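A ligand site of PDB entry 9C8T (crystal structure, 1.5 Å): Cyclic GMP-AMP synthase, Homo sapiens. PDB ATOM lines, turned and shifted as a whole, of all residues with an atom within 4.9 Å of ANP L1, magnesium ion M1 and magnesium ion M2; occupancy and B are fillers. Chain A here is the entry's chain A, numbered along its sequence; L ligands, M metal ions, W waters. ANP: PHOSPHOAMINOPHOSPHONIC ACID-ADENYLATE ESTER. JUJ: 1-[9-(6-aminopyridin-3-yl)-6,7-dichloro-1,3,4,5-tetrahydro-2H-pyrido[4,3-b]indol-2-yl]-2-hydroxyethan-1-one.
An oxygen (O2G) of ANP L1 lies within hydrogen-bond range of the side-chain hydroxyl (OG) of Ser 280.
OG of Ser 225 lies within hydrogen-bond range of O2' of ANP L1, 2.8 Å away.
An oxygen (O1G) of ANP L1 lies within salt-bridge range of the side-chain amino group (NZ) of Lys 259 (3.0 Å).
O1B of ANP L1 lies within salt-bridge range of NZ of Lys 284, 3.9 Å away.
OE1 of Glu 228 lies within hydrogen-bond range of O2' of ANP L1 (2.7 Å).
O1G of ANP L1 is in hydrogen-bond range of OG of Ser 58, at 2.6 Å.
An oxygen (O2B) of ANP L1 lies close to the backbone NH of Ser 58 (2.9 Å).
The backbone NH (N) of Asp 164 is in hydrogen-bond range of the backbone carbonyl oxygen (O) of Phe 71, at 2.9 Å.
NZ of Lys 284 is in salt-bridge range of OE2 of Glu 61.
The side-chain carboxylate (OE1) of Glu 228 is in salt-bridge range of the side-chain amino group (NZ) of Lys 284, 2.9 Å away.
The side-chain carboxylate (OE2) of Glu 228 is in hydrogen-bond range of the side-chain hydroxyl (OH) of Tyr 281 (2.7 Å).
The backbone carbonyl oxygen of Ser 58 is in hydrogen-bond range of the backbone NH of Lys 64 (3.1 Å).
The backbone NH (N) of Tyr 281 lies close to the side-chain hydroxyl (OG) of Ser 279 (3.1 Å).
CA of Gly 57 touches O2B of ANP L1, 3.4 Å away.
Lys 64 touches ANP L1 (CD to O1G, 3.8 Å).
Arg 221 touches ANP L1 (NH2 to N1, 3.7 Å).
CE2 of Tyr 281 touches N1 of ANP L1, 3.3 Å away.
Hydrophobic or aromatic side chains that line ANP L1: Tyr 281.
12 residues have an atom within 4 Å of ANP L1: Gly 57, Ser 58, Lys 64, Glu 70, Asp 72, Arg 221, Ser 225, Glu 228, Lys 259, Ser 280, Tyr 281 and Lys 284.
Within 4 Å of magnesium ion M1: Glu 70, Asp 72 and Asp 164.
The nearest printed residue that does not touch magnesium ion M1 is Phe 71 (4.8 Å).
Merely in contact with magnesium ion M2: Ser 58 (3.9 Å).
Within 4 Å of magnesium ion M2: Ser 58, Glu 70 and Asp 72.
Magnesium ion M1 is bound by the side-chain carboxylate (OD1) of Asp 72 (2.0 Å), the side-chain carboxylate (OE2) of Glu 70 (2.0 Å), the side-chain carboxylate (OD2) of Asp 164 (2.0 Å), an oxygen (O04) of JUJ L2 (2.1 Å), an oxygen (O2A) of ANP L1 (2.1 Å) and an oxygen (O01) of JUJ L2 (2.2 Å).
Magnesium ion M2 is bound by water W9 (2.0 Å), the side-chain carboxylate of Glu 70 (2.1 Å), an oxygen (O2B) of ANP L1 (2.1 Å), the side-chain carboxylate of Asp 72 (2.1 Å), an oxygen (O3G) of ANP L1 (2.1 Å) and an oxygen (O2A) of ANP L1 (2.1 Å).
Magnesium ion M2 has six donor atoms within binding distance.
Water W3 bridges N7 of ANP L1 (2.7 Å) and OG of Ser 279 (2.8 Å).
Water W4 lies within hydrogen-bond range of an oxygen (O1G) of ANP L1 (2.7 Å), the side-chain amino group of Lys 64 (3.0 Å) and the side-chain carboxylate of Glu 263 (3.4 Å).
Water W6 bridges the side-chain carboxylate (OE1) of Glu 61 (2.6 Å) and an oxygen (O1B) of ANP L1 (2.8 Å).
Water W8 lies within hydrogen-bond range of an oxygen (O1B) of ANP L1 (2.8 Å), the backbone NH (N) of Tyr 281 (3.1 Å) and the side-chain hydroxyl (OG) of Ser 280 (3.2 Å).
Water W5 lies within hydrogen-bond range of the side-chain hydroxyl (OG) of Ser 280 (2.9 Å), an oxygen (O1A) of ANP L1 (2.9 Å), the backbone NH (N) of Tyr 281 (3.0 Å) and the side-chain hydroxyl (OG) of Ser 279 (3.4 Å).
Water W10 bridges the side-chain amino group (NZ) of Lys 259 and a nitrogen (N3B) of ANP L1.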
ATOM      1  N   GLY A  57      26.731   3.626   2.005  1.00  0.00           N
ATOM      2  CA  GLY A  57      25.414   4.165   1.839  1.00  0.00           C
ATOM      3  C   GLY A  57      24.457   3.688   2.939  1.00  0.00           C
ATOM      4  O   GLY A  57      24.828   3.097   3.937  1.00  0.00           O
ATOM      5  N   SER A  58      23.170   4.099   2.755  1.00  0.00           N
ATOM      6  CA  SER A  58      22.243   4.128   3.867  1.00  0.00           C
ATOM      7  C   SER A  58      21.921   2.755   4.420  1.00  0.00           C
ATOM      8  O   SER A  58      21.645   2.633   5.607  1.00  0.00           O
ATOM      9  CB  SER A  58      20.962   4.856   3.541  1.00  0.00           C
ATOM     10  OG  SER A  58      20.274   4.167   2.498  1.00  0.00           O
ATOM     11  N   GLU A  61      24.663   1.923   6.768  1.00  0.00           N
ATOM     12  CA  GLU A  61      24.626   2.879   7.873  1.00  0.00           C
ATOM     13  C   GLU A  61      23.384   2.729   8.723  1.00  0.00           C
ATOM     14  O   GLU A  61      23.225   3.482   9.694  1.00  0.00           O
ATOM     15  CB  GLU A  61      24.664   4.324   7.348  1.00  0.00           C
ATOM     16  CG  GLU A  61      25.932   4.636   6.510  1.00  0.00           C
ATOM     17  CD  GLU A  61      25.740   5.849   5.624  1.00  0.00           C
ATOM     18  OE1 GLU A  61      24.566   6.245   5.366  1.00  0.00           O
ATOM     19  OE2 GLU A  61      26.781   6.374   5.155  1.00  0.00           O
ATOM     20  N   LYS A  64      18.656   3.512   6.000  1.00  0.00           N
ATOM     21  CA  LYS A  64      17.751   3.288   4.884  1.00  0.00           C
ATOM     22  C   LYS A  64      16.327   3.282   5.430  1.00  0.00           C
ATOM     23  O   LYS A  64      16.060   2.664   6.469  1.00  0.00           O
ATOM     24  CB  LYS A  64      18.099   1.938   4.228  1.00  0.00           C
ATOM     25  CG  LYS A  64      17.180   1.585   3.057  1.00  0.00           C
ATOM     26  CD  LYS A  64      17.683   2.323   1.791  1.00  0.00           C
ATOM     27  CE  LYS A  64      16.730   2.205   0.593  1.00  0.00           C
ATOM     28  NZ  LYS A  64      15.355   2.801   0.807  1.00  0.00           N
ATOM     29  N   GLU A  70      17.498  -0.328  -2.089  1.00  0.00           N
ATOM     30  CA  GLU A  70      18.573   0.412  -2.750  1.00  0.00           C
ATOM     31  C   GLU A  70      19.855   0.261  -1.947  1.00  0.00           C
ATOM     32  O   GLU A  70      19.919   0.628  -0.763  1.00  0.00           O
ATOM     33  CB  GLU A  70      18.224   1.875  -2.930  1.00  0.00           C
ATOM     34  CG  GLU A  70      19.037   2.500  -4.088  1.00  0.00           C
ATOM     35  CD  GLU A  70      20.292   3.236  -3.639  1.00  0.00           C
ATOM     36  OE1 GLU A  70      20.551   3.266  -2.445  1.00  0.00           O
ATOM     37  OE2 GLU A  70      20.971   3.823  -4.514  1.00  0.00           O
ATOM     38  N   PHE A  71      20.858  -0.330  -2.582  1.00  0.00           N
ATOM     39  CA  PHE A  71      22.101  -0.669  -1.928  1.00  0.00           C
ATOM     40  C   PHE A  71      23.272  -0.082  -2.699  1.00  0.00           C
ATOM     41  O   PHE A  71      23.217   0.007  -3.926  1.00  0.00           O
ATOM     42  CB  PHE A  71      22.296  -2.178  -1.987  1.00  0.00           C
ATOM     43  CG  PHE A  71      21.361  -2.960  -1.141  1.00  0.00           C
ATOM     44  CD1 PHE A  71      20.038  -3.158  -1.533  1.00  0.00           C
ATOM     45  CD2 PHE A  71      21.822  -3.548   0.044  1.00  0.00           C
ATOM     46  CE1 PHE A  71      19.158  -3.946  -0.725  1.00  0.00           C
ATOM     47  CE2 PHE A  71      20.938  -4.338   0.836  1.00  0.00           C
ATOM     48  CZ  PHE A  71      19.591  -4.484   0.432  1.00  0.00           C
ATOM     49  N   ASP A  72      24.307   0.338  -1.977  1.00  0.00           N
ATOM     50  CA  ASP A  72      25.459   1.038  -2.563  1.00  0.00           C
ATOM     51  C   ASP A  72      26.704   0.311  -2.180  1.00  0.00           C
ATOM     52  O   ASP A  72      26.978   0.106  -1.001  1.00  0.00           O
ATOM     53  CB  ASP A  72      25.499   2.454  -2.046  1.00  0.00           C
ATOM     54  CG  ASP A  72      24.260   3.173  -2.345  1.00  0.00           C
ATOM     55  OD1 ASP A  72      24.024   3.531  -3.526  1.00  0.00           O
ATOM     56  OD2 ASP A  72      23.484   3.409  -1.400  1.00  0.00           O
ATOM     57  N   ASP A 164      23.873   0.131  -6.703  1.00  0.00           N
ATOM     58  CA  ASP A 164      24.886   0.973  -7.323  1.00  0.00           C
ATOM     59  C   ASP A 164      26.240   0.344  -7.037  1.00  0.00           C
ATOM     60  O   ASP A 164      26.645   0.190  -5.860  1.00  0.00           O
ATOM     61  CB  ASP A 164      24.859   2.361  -6.696  1.00  0.00           C
ATOM     62  CG  ASP A 164      23.654   3.187  -7.129  1.00  0.00           C
ATOM     63  OD1 ASP A 164      23.319   3.171  -8.336  1.00  0.00           O
ATOM     64  OD2 ASP A 164      23.047   3.850  -6.282  1.00  0.00           O
ATOM     65  N   ARG A 221      36.774  11.583  -8.780  1.00  0.00           N
ATOM     66  CA  ARG A 221      36.227  12.378  -7.699  1.00  0.00           C
ATOM     67  C   ARG A 221      36.578  11.721  -6.366  1.00  0.00           C
ATOM     68  O   ARG A 221      36.435  10.507  -6.216  1.00  0.00           O
ATOM     69  CB  ARG A 221      34.741  12.484  -7.819  1.00  0.00           C
ATOM     70  CG  ARG A 221      34.212  13.162  -6.599  1.00  0.00           C
ATOM     71  CD  ARG A 221      33.023  13.903  -6.728  1.00  0.00           C
ATOM     72  NE  ARG A 221      32.858  14.584  -5.449  1.00  0.00           N
ATOM     73  CZ  ARG A 221      31.907  15.474  -5.240  1.00  0.00           C
ATOM     74  NH1 ARG A 221      31.089  15.857  -6.207  1.00  0.00           N
ATOM     75  NH2 ARG A 221      31.728  15.952  -4.008  1.00  0.00           N
ATOM     76  N   SER A 225      33.013   7.867   1.450  1.00  0.00           N
ATOM     77  CA  SER A 225      31.771   7.187   1.847  1.00  0.00           C
ATOM     78  C   SER A 225      32.034   6.202   2.985  1.00  0.00           C
ATOM     79  O   SER A 225      31.142   5.927   3.809  1.00  0.00           O
ATOM     80  CB  SER A 225      31.244   6.451   0.602  1.00  0.00           C
ATOM     81  OG  SER A 225      29.908   6.036   0.785  1.00  0.00           O
ATOM     82  N   GLU A 228      31.892   8.160   6.188  1.00  0.00           N
ATOM     83  CA  GLU A 228      30.497   8.463   6.544  1.00  0.00           C
ATOM     84  C   GLU A 228      29.856   7.285   7.245  1.00  0.00           C
ATOM     85  O   GLU A 228      29.158   7.450   8.244  1.00  0.00           O
ATOM     86  CB  GLU A 228      29.711   8.787   5.265  1.00  0.00           C
ATOM     87  CG  GLU A 228      30.291  10.059   4.611  1.00  0.00           C
ATOM     88  CD  GLU A 228      29.747  10.362   3.220  1.00  0.00           C
ATOM     89  OE1 GLU A 228      28.784   9.695   2.769  1.00  0.00           O
ATOM     90  OE2 GLU A 228      30.309  11.273   2.567  1.00  0.00           O
ATOM     91  N   LYS A 259      15.528  12.568   5.747  1.00  0.00           N
ATOM     92  CA  LYS A 259      15.507  11.837   4.483  1.00  0.00           C
ATOM     93  C   LYS A 259      14.073  11.669   3.996  1.00  0.00           C
ATOM     94  O   LYS A 259      13.819  11.821   2.811  1.00  0.00           O
ATOM     95  CB  LYS A 259      16.153  10.463   4.682  1.00  0.00           C
ATOM     96  CG  LYS A 259      17.695  10.595   4.757  1.00  0.00           C
ATOM     97  CD  LYS A 259      18.285   9.227   5.226  1.00  0.00           C
ATOM     98  CE  LYS A 259      17.855   8.095   4.273  1.00  0.00           C
ATOM     99  NZ  LYS A 259      18.510   8.421   3.018  1.00  0.00           N
ATOM    100  N   GLU A 263      12.405  13.011   0.575  1.00  0.00           N
ATOM    101  CA  GLU A 263      11.840  12.029  -0.343  1.00  0.00           C
ATOM    102  C   GLU A 263      10.396  12.362  -0.659  1.00  0.00           C
ATOM    103  O   GLU A 263       9.993  12.297  -1.814  1.00  0.00           O
ATOM    104  CB  GLU A 263      11.929  10.606   0.226  1.00  0.00           C
ATOM    105  CG  GLU A 263      13.285   9.923   0.057  1.00  0.00           C
ATOM    106  CD  GLU A 263      13.236   8.423   0.333  1.00  0.00           C
ATOM    107  OE1 GLU A 263      12.135   7.845   0.206  1.00  0.00           O
ATOM    108  OE2 GLU A 263      14.281   7.828   0.668  1.00  0.00           O
ATOM    109  N   SER A 279      19.246  15.915  -3.142  1.00  0.00           N
ATOM    110  CA  SER A 279      19.308  14.473  -2.917  1.00  0.00           C
ATOM    111  C   SER A 279      19.482  14.215  -1.433  1.00  0.00           C
ATOM    112  O   SER A 279      19.725  15.123  -0.637  1.00  0.00           O
ATOM    113  CB  SER A 279      20.464  13.820  -3.662  1.00  0.00           C
ATOM    114  OG  SER A 279      21.692  14.100  -3.010  1.00  0.00           O
ATOM    115  N   SER A 280      19.353  12.951  -1.048  1.00  0.00           N
ATOM    116  CA  SER A 280      19.542  12.647   0.348  1.00  0.00           C
ATOM    117  C   SER A 280      20.941  13.008   0.836  1.00  0.00           C
ATOM    118  O   SER A 280      21.115  13.185   2.036  1.00  0.00           O
ATOM    119  CB  SER A 280      19.224  11.166   0.600  1.00  0.00           C
ATOM    120  OG  SER A 280      20.122  10.347  -0.124  1.00  0.00           O
ATOM    121  N   TYR A 281      21.934  13.122  -0.044  1.00  0.00           N
ATOM    122  CA  TYR A 281      23.259  13.531   0.410  1.00  0.00           C
ATOM    123  C   TYR A 281      23.263  14.950   0.924  1.00  0.00           C
ATOM    124  O   TYR A 281      24.069  15.258   1.786  1.00  0.00           O
ATOM    125  CB  TYR A 281      24.287  13.364  -0.701  1.00  0.00           C
ATOM    126  CG  TYR A 281      25.694  13.435  -0.197  1.00  0.00           C
ATOM    127  CD1 TYR A 281      26.200  12.405   0.628  1.00  0.00           C
ATOM    128  CD2 TYR A 281      26.498  14.519  -0.467  1.00  0.00           C
ATOM    129  CE1 TYR A 281      27.505  12.443   1.102  1.00  0.00           C
ATOM    130  CE2 TYR A 281      27.852  14.560   0.029  1.00  0.00           C
ATOM    131  CZ  TYR A 281      28.305  13.525   0.814  1.00  0.00           C
ATOM    132  OH  TYR A 281      29.595  13.545   1.317  1.00  0.00           O
ATOM    133  N   LYS A 284      22.068  14.432   4.426  1.00  0.00           N
ATOM    134  CA  LYS A 284      23.097  13.753   5.198  1.00  0.00           C
ATOM    135  C   LYS A 284      24.215  14.715   5.585  1.00  0.00           C
ATOM    136  O   LYS A 284      24.692  14.685   6.720  1.00  0.00           O
ATOM    137  CB  LYS A 284      23.631  12.590   4.374  1.00  0.00           C
ATOM    138  CG  LYS A 284      24.546  11.684   5.108  1.00  0.00           C
ATOM    139  CD  LYS A 284      25.003  10.615   4.084  1.00  0.00           C
ATOM    140  CE  LYS A 284      25.766   9.509   4.805  1.00  0.00           C
ATOM    141  NZ  LYS A 284      26.351   8.505   3.766  1.00  0.00           N
ATOM    142  N   ASN A 327      30.688  20.549   1.845  1.00  0.00           N
ATOM    143  CA  ASN A 327      30.968  19.114   1.979  1.00  0.00           C
ATOM    144  C   ASN A 327      31.692  18.875   3.296  1.00  0.00           C
ATOM    145  O   ASN A 327      32.563  19.638   3.694  1.00  0.00           O
ATOM    146  CB  ASN A 327      31.824  18.672   0.773  1.00  0.00           C
ATOM    147  CG  ASN A 327      32.133  17.210   0.759  1.00  0.00           C
ATOM    148  OD1 ASN A 327      32.927  16.762   1.577  1.00  0.00           O
ATOM    149  ND2 ASN A 327      31.517  16.435  -0.167  1.00  0.00           N
HETATM  150  PG  ANP L   1      19.543   6.631   0.258  1.00  0.00           P
HETATM  151  O1G ANP L   1      18.770   5.965   1.375  1.00  0.00           O
HETATM  152  O2G ANP L   1      18.661   7.780  -0.384  1.00  0.00           O
HETATM  153  O3G ANP L   1      19.987   5.645  -0.789  1.00  0.00           O
HETATM  154  PB  ANP L   1      22.400   7.029   0.512  1.00  0.00           P
HETATM  155  O1B ANP L   1      23.399   7.692   1.403  1.00  0.00           O
HETATM  156  O2B ANP L   1      22.642   5.536   0.321  1.00  0.00           O
HETATM  157  N3B ANP L   1      20.887   7.283   1.041  1.00  0.00           N
HETATM  158  PA  ANP L   1      22.799   7.181  -2.359  1.00  0.00           P
HETATM  159  O1A ANP L   1      22.222   8.222  -3.263  1.00  0.00           O
HETATM  160  O2A ANP L   1      22.416   5.739  -2.640  1.00  0.00           O
HETATM  161  O3A ANP L   1      22.522   7.758  -0.910  1.00  0.00           O
HETATM  162  O5' ANP L   1      24.388   7.404  -2.484  1.00  0.00           O
HETATM  163  C5' ANP L   1      25.282   6.444  -1.918  1.00  0.00           C
HETATM  164  C4' ANP L   1      26.518   7.158  -1.396  1.00  0.00           C
HETATM  165  O4' ANP L   1      27.126   7.939  -2.448  1.00  0.00           O
HETATM  166  C3' ANP L   1      26.245   8.200  -0.307  1.00  0.00           C
HETATM  167  O3' ANP L   1      26.045   7.629   0.974  1.00  0.00           O
HETATM  168  C2' ANP L   1      27.494   9.067  -0.391  1.00  0.00           C
HETATM  169  O2' ANP L   1      28.580   8.489   0.315  1.00  0.00           O
HETATM  170  C1' ANP L   1      27.793   9.059  -1.893  1.00  0.00           C
HETATM  171  N9  ANP L   1      27.294  10.250  -2.545  1.00  0.00           N
HETATM  172  C8  ANP L   1      26.052  10.472  -3.103  1.00  0.00           C
HETATM  173  N7  ANP L   1      25.882  11.682  -3.576  1.00  0.00           N
HETATM  174  C5  ANP L   1      27.064  12.308  -3.271  1.00  0.00           C
HETATM  175  C6  ANP L   1      27.515  13.628  -3.509  1.00  0.00           C
HETATM  176  N6  ANP L   1      26.758  14.561  -4.076  1.00  0.00           N
HETATM  177  N1  ANP L   1      28.741  13.940  -3.068  1.00  0.00           N
HETATM  178  C2  ANP L   1      29.499  12.999  -2.495  1.00  0.00           C
HETATM  179  N3  ANP L   1      29.205  11.719  -2.246  1.00  0.00           N
HETATM  180  C4  ANP L   1      27.946  11.452  -2.641  1.00  0.00           C
HETATM  181  C13 JUJ L   2      24.677   8.703  -7.384  1.00  0.00           C
HETATM  182  C20 JUJ L   2      29.429   6.940  -4.464  1.00  0.00           C
HETATM  183  C21 JUJ L   2      28.995   5.966  -5.354  1.00  0.00           C
HETATM  184  C26 JUJ L   2      29.657   6.466  -3.137  1.00  0.00           C
HETATM  185  O01 JUJ L   2      21.714   6.331  -5.624  1.00  0.00           O
HETATM  186  C02 JUJ L   2      22.578   7.235  -6.262  1.00  0.00           C
HETATM  187  C03 JUJ L   2      24.009   6.963  -5.824  1.00  0.00           C
HETATM  188  O04 JUJ L   2      24.286   6.098  -5.049  1.00  0.00           O
HETATM  189  N05 JUJ L   2      24.929   7.706  -6.321  1.00  0.00           N
HETATM  190  C06 JUJ L   2      26.345   7.464  -6.031  1.00  0.00           C
HETATM  191  C07 JUJ L   2      27.177   8.767  -6.051  1.00  0.00           C
HETATM  192  C08 JUJ L   2      28.515   9.026  -5.543  1.00  0.00           C
HETATM  193  C09 JUJ L   2      28.720  10.435  -5.836  1.00  0.00           C
HETATM  194  N10 JUJ L   2      27.587  10.903  -6.489  1.00  0.00           N
HETATM  195  C11 JUJ L   2      26.675   9.886  -6.599  1.00  0.00           C
HETATM  196  C12 JUJ L   2      25.345  10.043  -7.212  1.00  0.00           C
HETATM  197  C14 JUJ L   2      29.852  11.055  -5.464  1.00  0.00           C
HETATM  198 CL2  JUJ L   2      30.026  12.777  -5.837  1.00  0.00          CL
HETATM  199  C16 JUJ L   2      30.815  10.368  -4.812  1.00  0.00           C
HETATM  200 CL1  JUJ L   2      32.251  11.154  -4.252  1.00  0.00          CL
HETATM  201  C18 JUJ L   2      30.661   9.019  -4.490  1.00  0.00           C
HETATM  202  C19 JUJ L   2      29.555   8.357  -4.840  1.00  0.00           C
HETATM  203  N22 JUJ L   2      28.855   4.644  -5.098  1.00  0.00           N
HETATM  204  C23 JUJ L   2      29.061   4.190  -3.804  1.00  0.00           C
HETATM  205  N24 JUJ L   2      28.881   2.862  -3.561  1.00  0.00           N
HETATM  206  C25 JUJ L   2      29.477   5.117  -2.808  1.00  0.00           C
HETATM  207 MG    MG M   1      22.765   4.787  -4.486  1.00  0.00          MG
HETATM  208 MG    MG M   2      21.674   4.416  -1.133  1.00  0.00          MG
HETATM  209  O   HOH W   1      27.383  17.800  -4.485  1.00  0.00           O
HETATM  210  O   HOH W   2      29.653  16.601  -2.412  1.00  0.00           O
HETATM  211  O   HOH W   3      23.408  12.384  -4.482  1.00  0.00           O
HETATM  212  O   HOH W   4      16.176   5.380   2.044  1.00  0.00           O
HETATM  213  O   HOH W   5      22.183  10.861  -2.034  1.00  0.00           O
HETATM  214  O   HOH W   6      22.843   7.775   4.103  1.00  0.00           O
HETATM  215  O   HOH W   7      19.458   8.666  -2.827  1.00  0.00           O
HETATM  216  O   HOH W   8      23.142  10.441   0.953  1.00  0.00           O
HETATM  217  O   HOH W   9      21.198   3.021   0.242  1.00  0.00           O
HETATM  218  O   HOH W  10      21.035   9.651   3.220  1.00  0.00           O
HETATM  219  O   HOH W  11      18.094   5.408  -2.752  1.00  0.00           O
HETATM  220  O   HOH W  12      31.054  10.041  -0.999  1.00  0.00           O
HETATM  221  O   HOH W  13      26.593  13.626  -7.268  1.00  0.00           O
HETATM  222  O   HOH W  14      16.486   9.119   1.313  1.00  0.00           O
